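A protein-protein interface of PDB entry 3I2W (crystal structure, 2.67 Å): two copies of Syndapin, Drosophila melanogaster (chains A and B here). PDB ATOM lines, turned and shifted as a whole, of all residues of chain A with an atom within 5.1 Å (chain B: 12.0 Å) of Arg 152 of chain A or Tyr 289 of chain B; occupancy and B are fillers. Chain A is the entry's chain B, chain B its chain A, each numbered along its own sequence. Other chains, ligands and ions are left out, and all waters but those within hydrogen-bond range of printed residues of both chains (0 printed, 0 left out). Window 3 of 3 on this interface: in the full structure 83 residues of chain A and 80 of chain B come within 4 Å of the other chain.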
ATOM      1  N   TYR A 144      22.337  12.752   0.880  1.00  0.00           N
ATOM      2  CA  TYR A 144      23.543  13.164   1.573  1.00  0.00           C
ATOM      3  C   TYR A 144      23.577  14.654   1.725  1.00  0.00           C
ATOM      4  O   TYR A 144      24.356  15.199   2.470  1.00  0.00           O
ATOM      5  CB  TYR A 144      24.777  12.700   0.820  1.00  0.00           C
ATOM      6  CG  TYR A 144      26.014  13.536   1.069  1.00  0.00           C
ATOM      7  CD1 TYR A 144      26.865  13.268   2.132  1.00  0.00           C
ATOM      8  CD2 TYR A 144      26.345  14.603   0.244  1.00  0.00           C
ATOM      9  CE1 TYR A 144      28.027  14.050   2.382  1.00  0.00           C
ATOM     10  CE2 TYR A 144      27.522  15.396   0.478  1.00  0.00           C
ATOM     11  CZ  TYR A 144      28.348  15.105   1.553  1.00  0.00           C
ATOM     12  OH  TYR A 144      29.487  15.861   1.800  1.00  0.00           O
ATOM     13  N   HIS A 145      22.734  15.337   0.991  1.00  0.00           N
ATOM     14  CA  HIS A 145      22.750  16.763   1.053  1.00  0.00           C
ATOM     15  C   HIS A 145      21.735  17.073   2.119  1.00  0.00           C
ATOM     16  O   HIS A 145      21.799  18.110   2.762  1.00  0.00           O
ATOM     17  CB  HIS A 145      22.344  17.393  -0.295  1.00  0.00           C
ATOM     18  CG  HIS A 145      23.462  17.519  -1.291  1.00  0.00           C
ATOM     19  ND1 HIS A 145      23.237  17.775  -2.626  1.00  0.00           N
ATOM     20  CD2 HIS A 145      24.808  17.430  -1.152  1.00  0.00           C
ATOM     21  CE1 HIS A 145      24.393  17.847  -3.267  1.00  0.00           C
ATOM     22  NE2 HIS A 145      25.365  17.640  -2.398  1.00  0.00           N
ATOM     23  N   CYS A 148      23.455  16.632   5.327  1.00  0.00           N
ATOM     24  CA  CYS A 148      24.337  17.762   5.607  1.00  0.00           C
ATOM     25  C   CYS A 148      23.539  18.904   6.193  1.00  0.00           C
ATOM     26  O   CYS A 148      23.963  19.557   7.157  1.00  0.00           O
ATOM     27  CB  CYS A 148      25.025  18.242   4.338  1.00  0.00           C
ATOM     28  SG  CYS A 148      26.499  17.341   3.903  1.00  0.00           S
ATOM     29  N   LYS A 149      22.386  19.143   5.577  1.00  0.00           N
ATOM     30  CA  LYS A 149      21.485  20.169   6.008  1.00  0.00           C
ATOM     31  C   LYS A 149      21.009  19.893   7.420  1.00  0.00           C
ATOM     32  O   LYS A 149      21.112  20.771   8.255  1.00  0.00           O
ATOM     33  CB  LYS A 149      20.301  20.290   5.052  1.00  0.00           C
ATOM     34  CG  LYS A 149      19.721  21.720   4.972  1.00  0.00           C
ATOM     35  CD  LYS A 149      18.399  21.792   4.183  1.00  0.00           C
ATOM     36  CE  LYS A 149      17.233  21.182   4.975  1.00  0.00           C
ATOM     37  NZ  LYS A 149      15.913  21.748   4.547  1.00  0.00           N
ATOM     38  N   THR A 150      20.498  18.697   7.694  1.00  0.00           N
ATOM     39  CA  THR A 150      20.058  18.384   9.050  1.00  0.00           C
ATOM     40  C   THR A 150      21.168  18.788  10.033  1.00  0.00           C
ATOM     41  O   THR A 150      21.037  19.752  10.802  1.00  0.00           O
ATOM     42  CB  THR A 150      19.700  16.885   9.267  1.00  0.00           C
ATOM     43  OG1 THR A 150      18.975  16.387   8.151  1.00  0.00           O
ATOM     44  CG2 THR A 150      18.828  16.715  10.502  1.00  0.00           C
ATOM     45  N   GLU A 151      22.275  18.068   9.974  1.00  0.00           N
ATOM     46  CA  GLU A 151      23.396  18.295  10.848  1.00  0.00           C
ATOM     47  C   GLU A 151      23.779  19.752  11.090  1.00  0.00           C
ATOM     48  O   GLU A 151      24.338  20.056  12.121  1.00  0.00           O
ATOM     49  CB  GLU A 151      24.587  17.522  10.306  1.00  0.00           C
ATOM     50  CG  GLU A 151      25.621  17.131  11.328  1.00  0.00           C
ATOM     51  CD  GLU A 151      26.895  17.915  11.167  1.00  0.00           C
ATOM     52  OE1 GLU A 151      26.841  19.170  11.231  1.00  0.00           O
ATOM     53  OE2 GLU A 151      27.948  17.261  10.968  1.00  0.00           O
ATOM     54  N   ARG A 152      23.496  20.657  10.169  1.00  0.00           N
ATOM     55  CA  ARG A 152      23.903  22.056  10.360  1.00  0.00           C
ATOM     56  C   ARG A 152      22.869  22.831  11.181  1.00  0.00           C
ATOM     57  O   ARG A 152      23.182  23.834  11.805  1.00  0.00           O
ATOM     58  CB  ARG A 152      24.173  22.733   9.012  1.00  0.00           C
ATOM     59  CG  ARG A 152      25.441  22.208   8.297  1.00  0.00           C
ATOM     60  CD  ARG A 152      25.682  22.894   6.926  1.00  0.00           C
ATOM     61  NE  ARG A 152      25.980  24.337   7.040  1.00  0.00           N
ATOM     62  CZ  ARG A 152      25.881  25.245   6.054  1.00  0.00           C
ATOM     63  NH1 ARG A 152      25.486  24.909   4.824  1.00  0.00           N
ATOM     64  NH2 ARG A 152      26.185  26.518   6.302  1.00  0.00           N
ATOM     65  N   SER A 153      21.636  22.340  11.177  1.00  0.00           N
ATOM     66  CA  SER A 153      20.533  22.978  11.871  1.00  0.00           C
ATOM     67  C   SER A 153      20.310  22.270  13.194  1.00  0.00           C
ATOM     68  O   SER A 153      19.484  22.695  14.007  1.00  0.00           O
ATOM     69  CB  SER A 153      19.268  22.867  11.038  1.00  0.00           C
ATOM     70  OG  SER A 153      18.822  21.532  11.057  1.00  0.00           O
ATOM     71  N   ALA A 154      21.031  21.174  13.394  1.00  0.00           N
ATOM     72  CA  ALA A 154      20.931  20.414  14.613  1.00  0.00           C
ATOM     73  C   ALA A 154      22.006  20.924  15.533  1.00  0.00           C
ATOM     74  O   ALA A 154      21.802  21.009  16.746  1.00  0.00           O
ATOM     75  CB  ALA A 154      21.109  18.924  14.341  1.00  0.00           C
ATOM     76  N   THR A 155      23.153  21.267  14.952  1.00  0.00           N
ATOM     77  CA  THR A 155      24.257  21.831  15.714  1.00  0.00           C
ATOM     78  C   THR A 155      23.911  23.256  16.073  1.00  0.00           C
ATOM     79  O   THR A 155      24.531  23.836  16.934  1.00  0.00           O
ATOM     80  CB  THR A 155      25.609  21.776  14.964  1.00  0.00           C
ATOM     81  OG1 THR A 155      25.395  22.066  13.589  1.00  0.00           O
ATOM     82  CG2 THR A 155      26.251  20.399  15.060  1.00  0.00           C
ATOM     83  N   ASN A 156      22.904  23.804  15.410  1.00  0.00           N
ATOM     84  CA  ASN A 156      22.323  25.074  15.789  1.00  0.00           C
ATOM     85  C   ASN A 156      21.472  25.048  17.037  1.00  0.00           C
ATOM     86  O   ASN A 156      21.592  25.936  17.895  1.00  0.00           O
ATOM     87  CB  ASN A 156      21.472  25.605  14.658  1.00  0.00           C
ATOM     88  CG  ASN A 156      22.187  26.646  13.865  1.00  0.00           C
ATOM     89  OD1 ASN A 156      23.228  27.158  14.300  1.00  0.00           O
ATOM     90  ND2 ASN A 156      21.650  26.979  12.690  1.00  0.00           N
ATOM     91  N   SER B 285      29.923  12.947 -10.914  1.00  0.00           N
ATOM     92  CA  SER B 285      31.082  13.431 -10.191  1.00  0.00           C
ATOM     93  C   SER B 285      30.531  13.716  -8.802  1.00  0.00           C
ATOM     94  O   SER B 285      29.367  14.112  -8.654  1.00  0.00           O
ATOM     95  CB  SER B 285      31.474  14.750 -10.834  1.00  0.00           C
ATOM     96  OG  SER B 285      30.263  15.429 -11.282  1.00  0.00           O
ATOM     97  N   PHE B 286      31.347  13.538  -7.775  1.00  0.00           N
ATOM     98  CA  PHE B 286      30.922  13.915  -6.447  1.00  0.00           C
ATOM     99  C   PHE B 286      30.679  15.432  -6.368  1.00  0.00           C
ATOM    100  O   PHE B 286      31.625  16.190  -6.517  1.00  0.00           O
ATOM    101  CB  PHE B 286      32.002  13.488  -5.465  1.00  0.00           C
ATOM    102  CG  PHE B 286      31.645  13.725  -4.039  1.00  0.00           C
ATOM    103  CD1 PHE B 286      31.116  12.707  -3.274  1.00  0.00           C
ATOM    104  CD2 PHE B 286      31.845  14.978  -3.459  1.00  0.00           C
ATOM    105  CE1 PHE B 286      30.789  12.922  -1.948  1.00  0.00           C
ATOM    106  CE2 PHE B 286      31.516  15.211  -2.128  1.00  0.00           C
ATOM    107  CZ  PHE B 286      30.983  14.179  -1.369  1.00  0.00           C
ATOM    108  N   VAL B 287      29.435  15.872  -6.164  1.00  0.00           N
ATOM    109  CA  VAL B 287      29.212  17.284  -5.874  1.00  0.00           C
ATOM    110  C   VAL B 287      29.004  17.551  -4.387  1.00  0.00           C
ATOM    111  O   VAL B 287      28.162  16.923  -3.731  1.00  0.00           O
ATOM    112  CB  VAL B 287      28.106  17.948  -6.745  1.00  0.00           C
ATOM    113  CG1 VAL B 287      26.766  17.273  -6.583  1.00  0.00           C
ATOM    114  CG2 VAL B 287      27.972  19.434  -6.424  1.00  0.00           C
ATOM    115  N   GLU B 288      29.800  18.483  -3.868  1.00  0.00           N
ATOM    116  CA  GLU B 288      29.762  18.905  -2.471  1.00  0.00           C
ATOM    117  C   GLU B 288      28.458  19.608  -2.022  1.00  0.00           C
ATOM    118  O   GLU B 288      27.466  19.721  -2.767  1.00  0.00           O
ATOM    119  CB  GLU B 288      30.989  19.777  -2.162  1.00  0.00           C
ATOM    120  CG  GLU B 288      31.444  19.769  -0.681  1.00  0.00           C
ATOM    121  CD  GLU B 288      31.113  18.452   0.069  1.00  0.00           C
ATOM    122  OE1 GLU B 288      31.992  17.573   0.181  1.00  0.00           O
ATOM    123  OE2 GLU B 288      29.976  18.282   0.564  1.00  0.00           O
ATOM    124  N   TYR B 289      28.457  20.066  -0.781  1.00  0.00           N
ATOM    125  CA  TYR B 289      27.261  20.632  -0.211  1.00  0.00           C
ATOM    126  C   TYR B 289      27.368  22.148  -0.198  1.00  0.00           C
ATOM    127  O   TYR B 289      28.439  22.662   0.102  1.00  0.00           O
ATOM    128  CB  TYR B 289      27.047  20.082   1.205  1.00  0.00           C
ATOM    129  CG  TYR B 289      25.851  20.692   1.842  1.00  0.00           C
ATOM    130  CD1 TYR B 289      24.571  20.420   1.349  1.00  0.00           C
ATOM    131  CD2 TYR B 289      25.986  21.591   2.893  1.00  0.00           C
ATOM    132  CE1 TYR B 289      23.455  21.010   1.903  1.00  0.00           C
ATOM    133  CE2 TYR B 289      24.878  22.189   3.455  1.00  0.00           C
ATOM    134  CZ  TYR B 289      23.620  21.894   2.959  1.00  0.00           C
ATOM    135  OH  TYR B 289      22.515  22.480   3.522  1.00  0.00           O
ATOM    136  N   THR B 290      26.281  22.851  -0.549  1.00  0.00           N
ATOM    137  CA  THR B 290      26.159  24.317  -0.311  1.00  0.00           C
ATOM    138  C   THR B 290      26.865  24.725   0.996  1.00  0.00           C
ATOM    139  O   THR B 290      27.434  25.818   1.108  1.00  0.00           O
ATOM    140  CB  THR B 290      24.645  24.811  -0.296  1.00  0.00           C
ATOM    141  OG1 THR B 290      24.283  25.292  -1.595  1.00  0.00           O
ATOM    142  CG2 THR B 290      24.370  25.957   0.750  1.00  0.00           C
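NE2 of His 145 of chain A sits at hydrogen-bond distance from O of Val 287 of chain B, 3.2 Å away.
OH of Tyr 144 of chain A lies within hydrogen-bond range of OE2 of Glu 288 of chain B, at 2.8 Å.
The backbone carbonyl oxygen (O) of Glu 288 of chain B sits at hydrogen-bond distance from a ring nitrogen (NE2) of His 145 of chain A (3.0 Å).
The backbone carbonyl oxygen (O) of Tyr 144 of chain A sits at hydrogen-bond distance from the side-chain sulfur (SG) of Cys 148 of chain A, 3.4 Å away.
The backbone carbonyl oxygen of Arg 152 of chain A sits at hydrogen-bond distance from the side-chain hydroxyl of Thr 155 of chain A (3.3 Å).
Among the printed residues, pairs that only touch across the chains: Tyr 144 of chain A with Phe 286 of chain B (3.9 Å), His 145 of chain A with Tyr 289 of chain B (3.4 Å), Cys 148 of chain A with Tyr 289 of chain B (3.6 Å), Lys 149 of chain A with Tyr 289 of chain B (3.2 Å) and Arg 152 of chain A with Tyr 289 of chain B (3.1 Å).
Arg 152 of chain A touches one residue of chain B.
Of chain A, only His 145, Cys 148, Lys 149 and Arg 152 come within 4 Å of Tyr 289 of chain B.
Lys 149 of chain A touches just one residue of chain B: Tyr 289.
No residue of chain B comes within 4 Å of Ser 153 of chain A.
No residue of chain B comes within 4 Å of Ala 154 of chain A.
No residue of chain B comes within 4 Å of Asn 156 of chain A.
Printed residues of chain A within 4 Å of Phe 286 of chain B: Tyr 144 (3.9 Å).
Of the printed residues of chain A, Glu 288 of chain B touches Tyr 144 (2.8 Å) and His 145 (3.0 Å).
Of the printed residues of chain B, Tyr 144 of chain A touches Phe 286 (3.9 Å) and Glu 288 (2.8 Å).
Of the printed residues of chain A, Val 287 of chain B touches His 145 (3.2 Å).
The nearest residue of chain A that does not touch Tyr 289 of chain B is Tyr 144 of chain A (4.8 Å).
Of the 11 printed residues of chain A, 5 touch a printed residue of chain B.
Among the printed residues, no Asp or Glu carboxylate lies within 4 Å of a Lys or Arg side-chain nitrogen of the other chain.
No position is printed for both chains.
Of the 8 pairs that touch across the chains among the printed residues, none has its exchanged pair printed and touching as well.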
